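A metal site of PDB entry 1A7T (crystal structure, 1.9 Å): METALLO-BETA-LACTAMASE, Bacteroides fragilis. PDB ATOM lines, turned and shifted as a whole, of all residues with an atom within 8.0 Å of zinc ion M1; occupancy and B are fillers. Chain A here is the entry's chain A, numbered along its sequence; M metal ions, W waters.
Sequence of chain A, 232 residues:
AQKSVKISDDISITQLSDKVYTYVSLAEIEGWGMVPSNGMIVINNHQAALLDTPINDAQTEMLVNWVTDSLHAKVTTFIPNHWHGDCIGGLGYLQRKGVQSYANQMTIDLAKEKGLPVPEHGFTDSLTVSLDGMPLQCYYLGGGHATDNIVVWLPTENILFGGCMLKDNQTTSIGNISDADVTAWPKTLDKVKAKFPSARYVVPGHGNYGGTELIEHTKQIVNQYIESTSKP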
ATOM      1  N   ASP A  52      10.815   1.752 -14.456  1.00  0.00           N
ATOM      2  CA  ASP A  52      11.713   1.884 -13.363  1.00  0.00           C
ATOM      3  C   ASP A  52      11.391   3.154 -12.568  1.00  0.00           C
ATOM      4  O   ASP A  52      10.936   4.203 -13.057  1.00  0.00           O
ATOM      5  CB  ASP A  52      13.219   2.018 -13.714  1.00  0.00           C
ATOM      6  CG  ASP A  52      13.878   0.707 -14.091  1.00  0.00           C
ATOM      7  OD1 ASP A  52      13.224  -0.348 -14.185  1.00  0.00           O
ATOM      8  OD2 ASP A  52      15.100   0.631 -14.287  1.00  0.00           O
ATOM      9  N   ASN A  81      12.623  -2.964 -14.318  1.00  0.00           N
ATOM     10  CA  ASN A  81      13.526  -3.816 -15.066  1.00  0.00           C
ATOM     11  C   ASN A  81      13.961  -5.064 -14.309  1.00  0.00           C
ATOM     12  O   ASN A  81      14.152  -6.084 -14.915  1.00  0.00           O
ATOM     13  CB  ASN A  81      14.779  -3.036 -15.387  1.00  0.00           C
ATOM     14  CG  ASN A  81      15.640  -3.782 -16.349  1.00  0.00           C
ATOM     15  OD1 ASN A  81      16.676  -4.316 -15.980  1.00  0.00           O
ATOM     16  ND2 ASN A  81      15.181  -3.885 -17.616  1.00  0.00           N
ATOM     17  N   HIS A  82      14.189  -4.997 -12.994  1.00  0.00           N
ATOM     18  CA  HIS A  82      14.610  -6.128 -12.197  1.00  0.00           C
ATOM     19  C   HIS A  82      14.408  -5.743 -10.713  1.00  0.00           C
ATOM     20  O   HIS A  82      13.793  -4.674 -10.487  1.00  0.00           O
ATOM     21  CB  HIS A  82      16.030  -6.633 -12.433  1.00  0.00           C
ATOM     22  CG  HIS A  82      17.131  -5.612 -12.329  1.00  0.00           C
ATOM     23  ND1 HIS A  82      17.328  -4.595 -13.259  1.00  0.00           N
ATOM     24  CD2 HIS A  82      18.091  -5.474 -11.417  1.00  0.00           C
ATOM     25  CE1 HIS A  82      18.382  -3.865 -12.904  1.00  0.00           C
ATOM     26  NE2 HIS A  82      18.834  -4.376 -11.765  1.00  0.00           N
ATOM     27  N   TRP A  83      14.780  -6.511  -9.725  1.00  0.00           N
ATOM     28  CA  TRP A  83      14.471  -6.137  -8.338  1.00  0.00           C
ATOM     29  C   TRP A  83      15.347  -5.192  -7.591  1.00  0.00           C
ATOM     30  O   TRP A  83      15.057  -4.844  -6.408  1.00  0.00           O
ATOM     31  CB  TRP A  83      14.382  -7.448  -7.504  1.00  0.00           C
ATOM     32  CG  TRP A  83      15.755  -8.083  -7.360  1.00  0.00           C
ATOM     33  CD1 TRP A  83      16.399  -8.883  -8.214  1.00  0.00           C
ATOM     34  CD2 TRP A  83      16.608  -7.955  -6.192  1.00  0.00           C
ATOM     35  NE1 TRP A  83      17.637  -9.258  -7.705  1.00  0.00           N
ATOM     36  CE2 TRP A  83      17.761  -8.726  -6.435  1.00  0.00           C
ATOM     37  CE3 TRP A  83      16.519  -7.237  -4.993  1.00  0.00           C
ATOM     38  CZ2 TRP A  83      18.780  -8.808  -5.490  1.00  0.00           C
ATOM     39  CZ3 TRP A  83      17.529  -7.323  -4.047  1.00  0.00           C
ATOM     40  CH2 TRP A  83      18.664  -8.113  -4.315  1.00  0.00           C
ATOM     41  N   HIS A  84      16.414  -4.651  -8.214  1.00  0.00           N
ATOM     42  CA  HIS A  84      17.282  -3.718  -7.485  1.00  0.00           C
ATOM     43  C   HIS A  84      16.638  -2.376  -7.226  1.00  0.00           C
ATOM     44  O   HIS A  84      15.595  -2.008  -7.789  1.00  0.00           O
ATOM     45  CB  HIS A  84      18.633  -3.546  -8.136  1.00  0.00           C
ATOM     46  CG  HIS A  84      19.578  -4.686  -8.181  1.00  0.00           C
ATOM     47  ND1 HIS A  84      20.576  -4.790  -9.105  1.00  0.00           N
ATOM     48  CD2 HIS A  84      19.680  -5.814  -7.452  1.00  0.00           C
ATOM     49  CE1 HIS A  84      21.314  -5.902  -8.945  1.00  0.00           C
ATOM     50  NE2 HIS A  84      20.786  -6.520  -7.914  1.00  0.00           N
ATOM     51  N   GLY A  85      17.273  -1.620  -6.267  1.00  0.00           N
ATOM     52  CA  GLY A  85      16.731  -0.358  -5.833  1.00  0.00           C
ATOM     53  C   GLY A  85      16.613   0.678  -6.913  1.00  0.00           C
ATOM     54  O   GLY A  85      15.724   1.533  -6.821  1.00  0.00           O
ATOM     55  N   ASP A  86      17.516   0.647  -7.892  1.00  0.00           N
ATOM     56  CA  ASP A  86      17.379   1.630  -8.963  1.00  0.00           C
ATOM     57  C   ASP A  86      16.272   1.257  -9.951  1.00  0.00           C
ATOM     58  O   ASP A  86      16.192   1.871 -11.006  1.00  0.00           O
ATOM     59  CB  ASP A  86      18.693   1.815  -9.685  1.00  0.00           C
ATOM     60  CG  ASP A  86      19.387   0.538 -10.106  1.00  0.00           C
ATOM     61  OD1 ASP A  86      19.516  -0.448  -9.356  1.00  0.00           O
ATOM     62  OD2 ASP A  86      19.791   0.514 -11.334  1.00  0.00           O
ATOM     63  N   CYS A  87      15.445   0.267  -9.702  1.00  0.00           N
ATOM     64  CA  CYS A  87      14.317  -0.142 -10.462  1.00  0.00           C
ATOM     65  C   CYS A  87      13.004  -0.067  -9.690  1.00  0.00           C
ATOM     66  O   CYS A  87      12.006   0.335 -10.222  1.00  0.00           O
ATOM     67  CB  CYS A  87      14.436  -1.595 -10.991  1.00  0.00           C
ATOM     68  SG  CYS A  87      16.011  -1.843 -11.867  1.00  0.00           S
ATOM     69  N   HIS A 145      22.769  -8.888 -16.161  1.00  0.00           N
ATOM     70  CA  HIS A 145      23.193  -8.099 -15.009  1.00  0.00           C
ATOM     71  C   HIS A 145      22.542  -8.594 -13.731  1.00  0.00           C
ATOM     72  O   HIS A 145      23.106  -8.623 -12.623  1.00  0.00           O
ATOM     73  CB  HIS A 145      22.851  -6.608 -15.223  1.00  0.00           C
ATOM     74  CG  HIS A 145      22.677  -5.895 -13.929  1.00  0.00           C
ATOM     75  ND1 HIS A 145      23.744  -5.328 -13.264  1.00  0.00           N
ATOM     76  CD2 HIS A 145      21.588  -5.592 -13.193  1.00  0.00           C
ATOM     77  CE1 HIS A 145      23.343  -4.723 -12.132  1.00  0.00           C
ATOM     78  NE2 HIS A 145      22.053  -4.876 -12.065  1.00  0.00           N
ATOM     79  N   ALA A 146      21.281  -8.967 -13.857  1.00  0.00           N
ATOM     80  CA  ALA A 146      20.521  -9.566 -12.759  1.00  0.00           C
ATOM     81  C   ALA A 146      19.878 -10.833 -13.328  1.00  0.00           C
ATOM     82  O   ALA A 146      19.650 -10.945 -14.550  1.00  0.00           O
ATOM     83  CB  ALA A 146      19.466  -8.645 -12.184  1.00  0.00           C
ATOM     84  N   ASP A 148      16.818 -11.789 -13.265  1.00  0.00           N
ATOM     85  CA  ASP A 148      15.444 -11.556 -13.693  1.00  0.00           C
ATOM     86  C   ASP A 148      15.281 -10.347 -14.617  1.00  0.00           C
ATOM     87  O   ASP A 148      14.136 -10.049 -14.932  1.00  0.00           O
ATOM     88  CB  ASP A 148      14.684 -11.272 -12.356  1.00  0.00           C
ATOM     89  CG  ASP A 148      15.161 -10.053 -11.614  1.00  0.00           C
ATOM     90  OD1 ASP A 148      16.358  -9.779 -11.389  1.00  0.00           O
ATOM     91  OD2 ASP A 148      14.352  -9.216 -11.136  1.00  0.00           O
ATOM     92  N   ASN A 149      16.358  -9.722 -15.047  1.00  0.00           N
ATOM     93  CA  ASN A 149      16.306  -8.534 -15.861  1.00  0.00           C
ATOM     94  C   ASN A 149      15.515  -8.763 -17.148  1.00  0.00           C
ATOM     95  O   ASN A 149      15.681  -9.793 -17.806  1.00  0.00           O
ATOM     96  CB  ASN A 149      17.637  -7.897 -16.166  1.00  0.00           C
ATOM     97  CG  ASN A 149      18.676  -8.792 -16.774  1.00  0.00           C
ATOM     98  OD1 ASN A 149      19.911  -8.516 -16.590  1.00  0.00           O
ATOM     99  ND2 ASN A 149      18.383  -9.818 -17.474  1.00  0.00           N
ATOM    100  N   GLY A 163      17.690  -1.429 -19.923  1.00  0.00           N
ATOM    101  CA  GLY A 163      17.958  -1.591 -18.487  1.00  0.00           C
ATOM    102  C   GLY A 163      19.400  -1.899 -18.209  1.00  0.00           C
ATOM    103  O   GLY A 163      20.302  -1.842 -19.060  1.00  0.00           O
ATOM    104  N   CYS A 164      19.691  -2.337 -16.954  1.00  0.00           N
ATOM    105  CA  CYS A 164      21.024  -2.634 -16.545  1.00  0.00           C
ATOM    106  C   CYS A 164      21.786  -3.743 -17.222  1.00  0.00           C
ATOM    107  O   CYS A 164      23.024  -3.727 -17.067  1.00  0.00           O
ATOM    108  CB  CYS A 164      21.059  -2.811 -15.006  1.00  0.00           C
ATOM    109  SG  CYS A 164      20.374  -1.255 -14.317  1.00  0.00           S
ATOM    110  N   MET A 165      21.139  -4.629 -17.960  1.00  0.00           N
ATOM    111  CA  MET A 165      21.891  -5.656 -18.689  1.00  0.00           C
ATOM    112  C   MET A 165      22.728  -4.985 -19.791  1.00  0.00           C
ATOM    113  O   MET A 165      23.682  -5.568 -20.319  1.00  0.00           O
ATOM    114  CB  MET A 165      20.941  -6.696 -19.317  1.00  0.00           C
ATOM    115  CG  MET A 165      20.421  -6.246 -20.671  1.00  0.00           C
ATOM    116  SD  MET A 165      19.633  -7.583 -21.585  1.00  0.00           S
ATOM    117  CE  MET A 165      18.161  -7.871 -20.573  1.00  0.00           C
ATOM    118  N   LYS A 167      25.348  -1.698 -20.751  1.00  0.00           N
ATOM    119  CA  LYS A 167      26.248  -0.669 -20.293  1.00  0.00           C
ATOM    120  C   LYS A 167      26.319   0.446 -21.352  1.00  0.00           C
ATOM    121  O   LYS A 167      26.179   0.252 -22.592  1.00  0.00           O
ATOM    122  CB  LYS A 167      27.638  -1.206 -20.015  1.00  0.00           C
ATOM    123  CG  LYS A 167      27.808  -2.395 -19.055  1.00  0.00           C
ATOM    124  CD  LYS A 167      27.255  -2.056 -17.719  1.00  0.00           C
ATOM    125  CE  LYS A 167      27.355  -3.217 -16.688  1.00  0.00           C
ATOM    126  NZ  LYS A 167      27.161  -2.546 -15.357  1.00  0.00           N
ATOM    127  N   ASN A 176      28.725  -4.079 -10.933  1.00  0.00           N
ATOM    128  CA  ASN A 176      28.148  -4.905  -9.889  1.00  0.00           C
ATOM    129  C   ASN A 176      27.592  -6.225 -10.402  1.00  0.00           C
ATOM    130  O   ASN A 176      26.576  -6.216 -11.147  1.00  0.00           O
ATOM    131  CB  ASN A 176      26.971  -4.050  -9.294  1.00  0.00           C
ATOM    132  CG  ASN A 176      26.324  -4.899  -8.190  1.00  0.00           C
ATOM    133  OD1 ASN A 176      27.018  -5.736  -7.591  1.00  0.00           O
ATOM    134  ND2 ASN A 176      25.022  -4.660  -8.050  1.00  0.00           N
ATOM    135  N   SER A 178      26.883  -9.009  -8.362  1.00  0.00           N
ATOM    136  CA  SER A 178      26.476  -9.815  -7.211  1.00  0.00           C
ATOM    137  C   SER A 178      25.190 -10.575  -7.500  1.00  0.00           C
ATOM    138  O   SER A 178      25.031 -11.596  -6.802  1.00  0.00           O
ATOM    139  CB  SER A 178      26.429  -8.918  -6.004  1.00  0.00           C
ATOM    140  OG  SER A 178      25.380  -7.933  -6.183  1.00  0.00           O
ATOM    141  N   ASP A 179      24.309 -10.226  -8.424  1.00  0.00           N
ATOM    142  CA  ASP A 179      23.109 -10.986  -8.730  1.00  0.00           C
ATOM    143  C   ASP A 179      23.064 -11.336 -10.206  1.00  0.00           C
ATOM    144  O   ASP A 179      22.025 -11.653 -10.730  1.00  0.00           O
ATOM    145  CB  ASP A 179      21.850 -10.120  -8.476  1.00  0.00           C
ATOM    146  CG  ASP A 179      21.924  -9.650  -7.034  1.00  0.00           C
ATOM    147  OD1 ASP A 179      21.987 -10.659  -6.288  1.00  0.00           O
ATOM    148  OD2 ASP A 179      22.014  -8.528  -6.551  1.00  0.00           O
ATOM    149  N   GLY A 205      20.565   1.087 -18.150  1.00  0.00           N
ATOM    150  CA  GLY A 205      20.206   1.296 -16.788  1.00  0.00           C
ATOM    151  C   GLY A 205      20.922   2.503 -16.192  1.00  0.00           C
ATOM    152  O   GLY A 205      20.334   3.147 -15.350  1.00  0.00           O
ATOM    153  N   HIS A 206      22.130   2.781 -16.643  1.00  0.00           N
ATOM    154  CA  HIS A 206      22.913   3.907 -16.153  1.00  0.00           C
ATOM    155  C   HIS A 206      23.747   4.528 -17.289  1.00  0.00           C
ATOM    156  O   HIS A 206      24.315   3.785 -18.115  1.00  0.00           O
ATOM    157  CB  HIS A 206      23.916   3.458 -15.067  1.00  0.00           C
ATOM    158  CG  HIS A 206      23.292   2.682 -13.959  1.00  0.00           C
ATOM    159  ND1 HIS A 206      22.699   3.267 -12.848  1.00  0.00           N
ATOM    160  CD2 HIS A 206      23.102   1.320 -13.828  1.00  0.00           C
ATOM    161  CE1 HIS A 206      22.166   2.336 -12.083  1.00  0.00           C
ATOM    162  NE2 HIS A 206      22.389   1.158 -12.649  1.00  0.00           N
HETATM  163 ZN    ZN M   1      20.680  -3.868 -10.915  1.00  0.00          ZN
HETATM  164 ZN    ZN M   2      21.334  -0.771 -12.380  1.00  0.00          ZN
HETATM  165  O   HOH W   1      21.264  -2.041 -10.650  1.00  0.00           O
HETATM  166  O   HOH W   2      23.421  -2.655  -9.225  1.00  0.00           O
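Zinc ion M1 is bound by water W1, 1.9 Å away. ND1 of His 84 binds zinc ion M1, at 2.0 Å. Zinc ion M1 is bound by a ring nitrogen (NE2) of His 145, 2.1 Å away. A ring nitrogen (NE2) of His 82 binds zinc ion M1.
Asp 86 touches zinc ion M1.
OD1 of Asn 81 sits at hydrogen-bond distance from ND1 of His 82 (2.8 Å). A ring nitrogen (NE2) of His 84 is in hydrogen-bond range of the side-chain carboxylate (OD2) of Asp 179. A ring nitrogen (ND1) of His 82 lies close to the side-chain sulfur (SG) of Cys 87 (3.4 Å). The backbone NH of His 145 lies within hydrogen-bond range of the side-chain amide oxygen of Asn 149.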
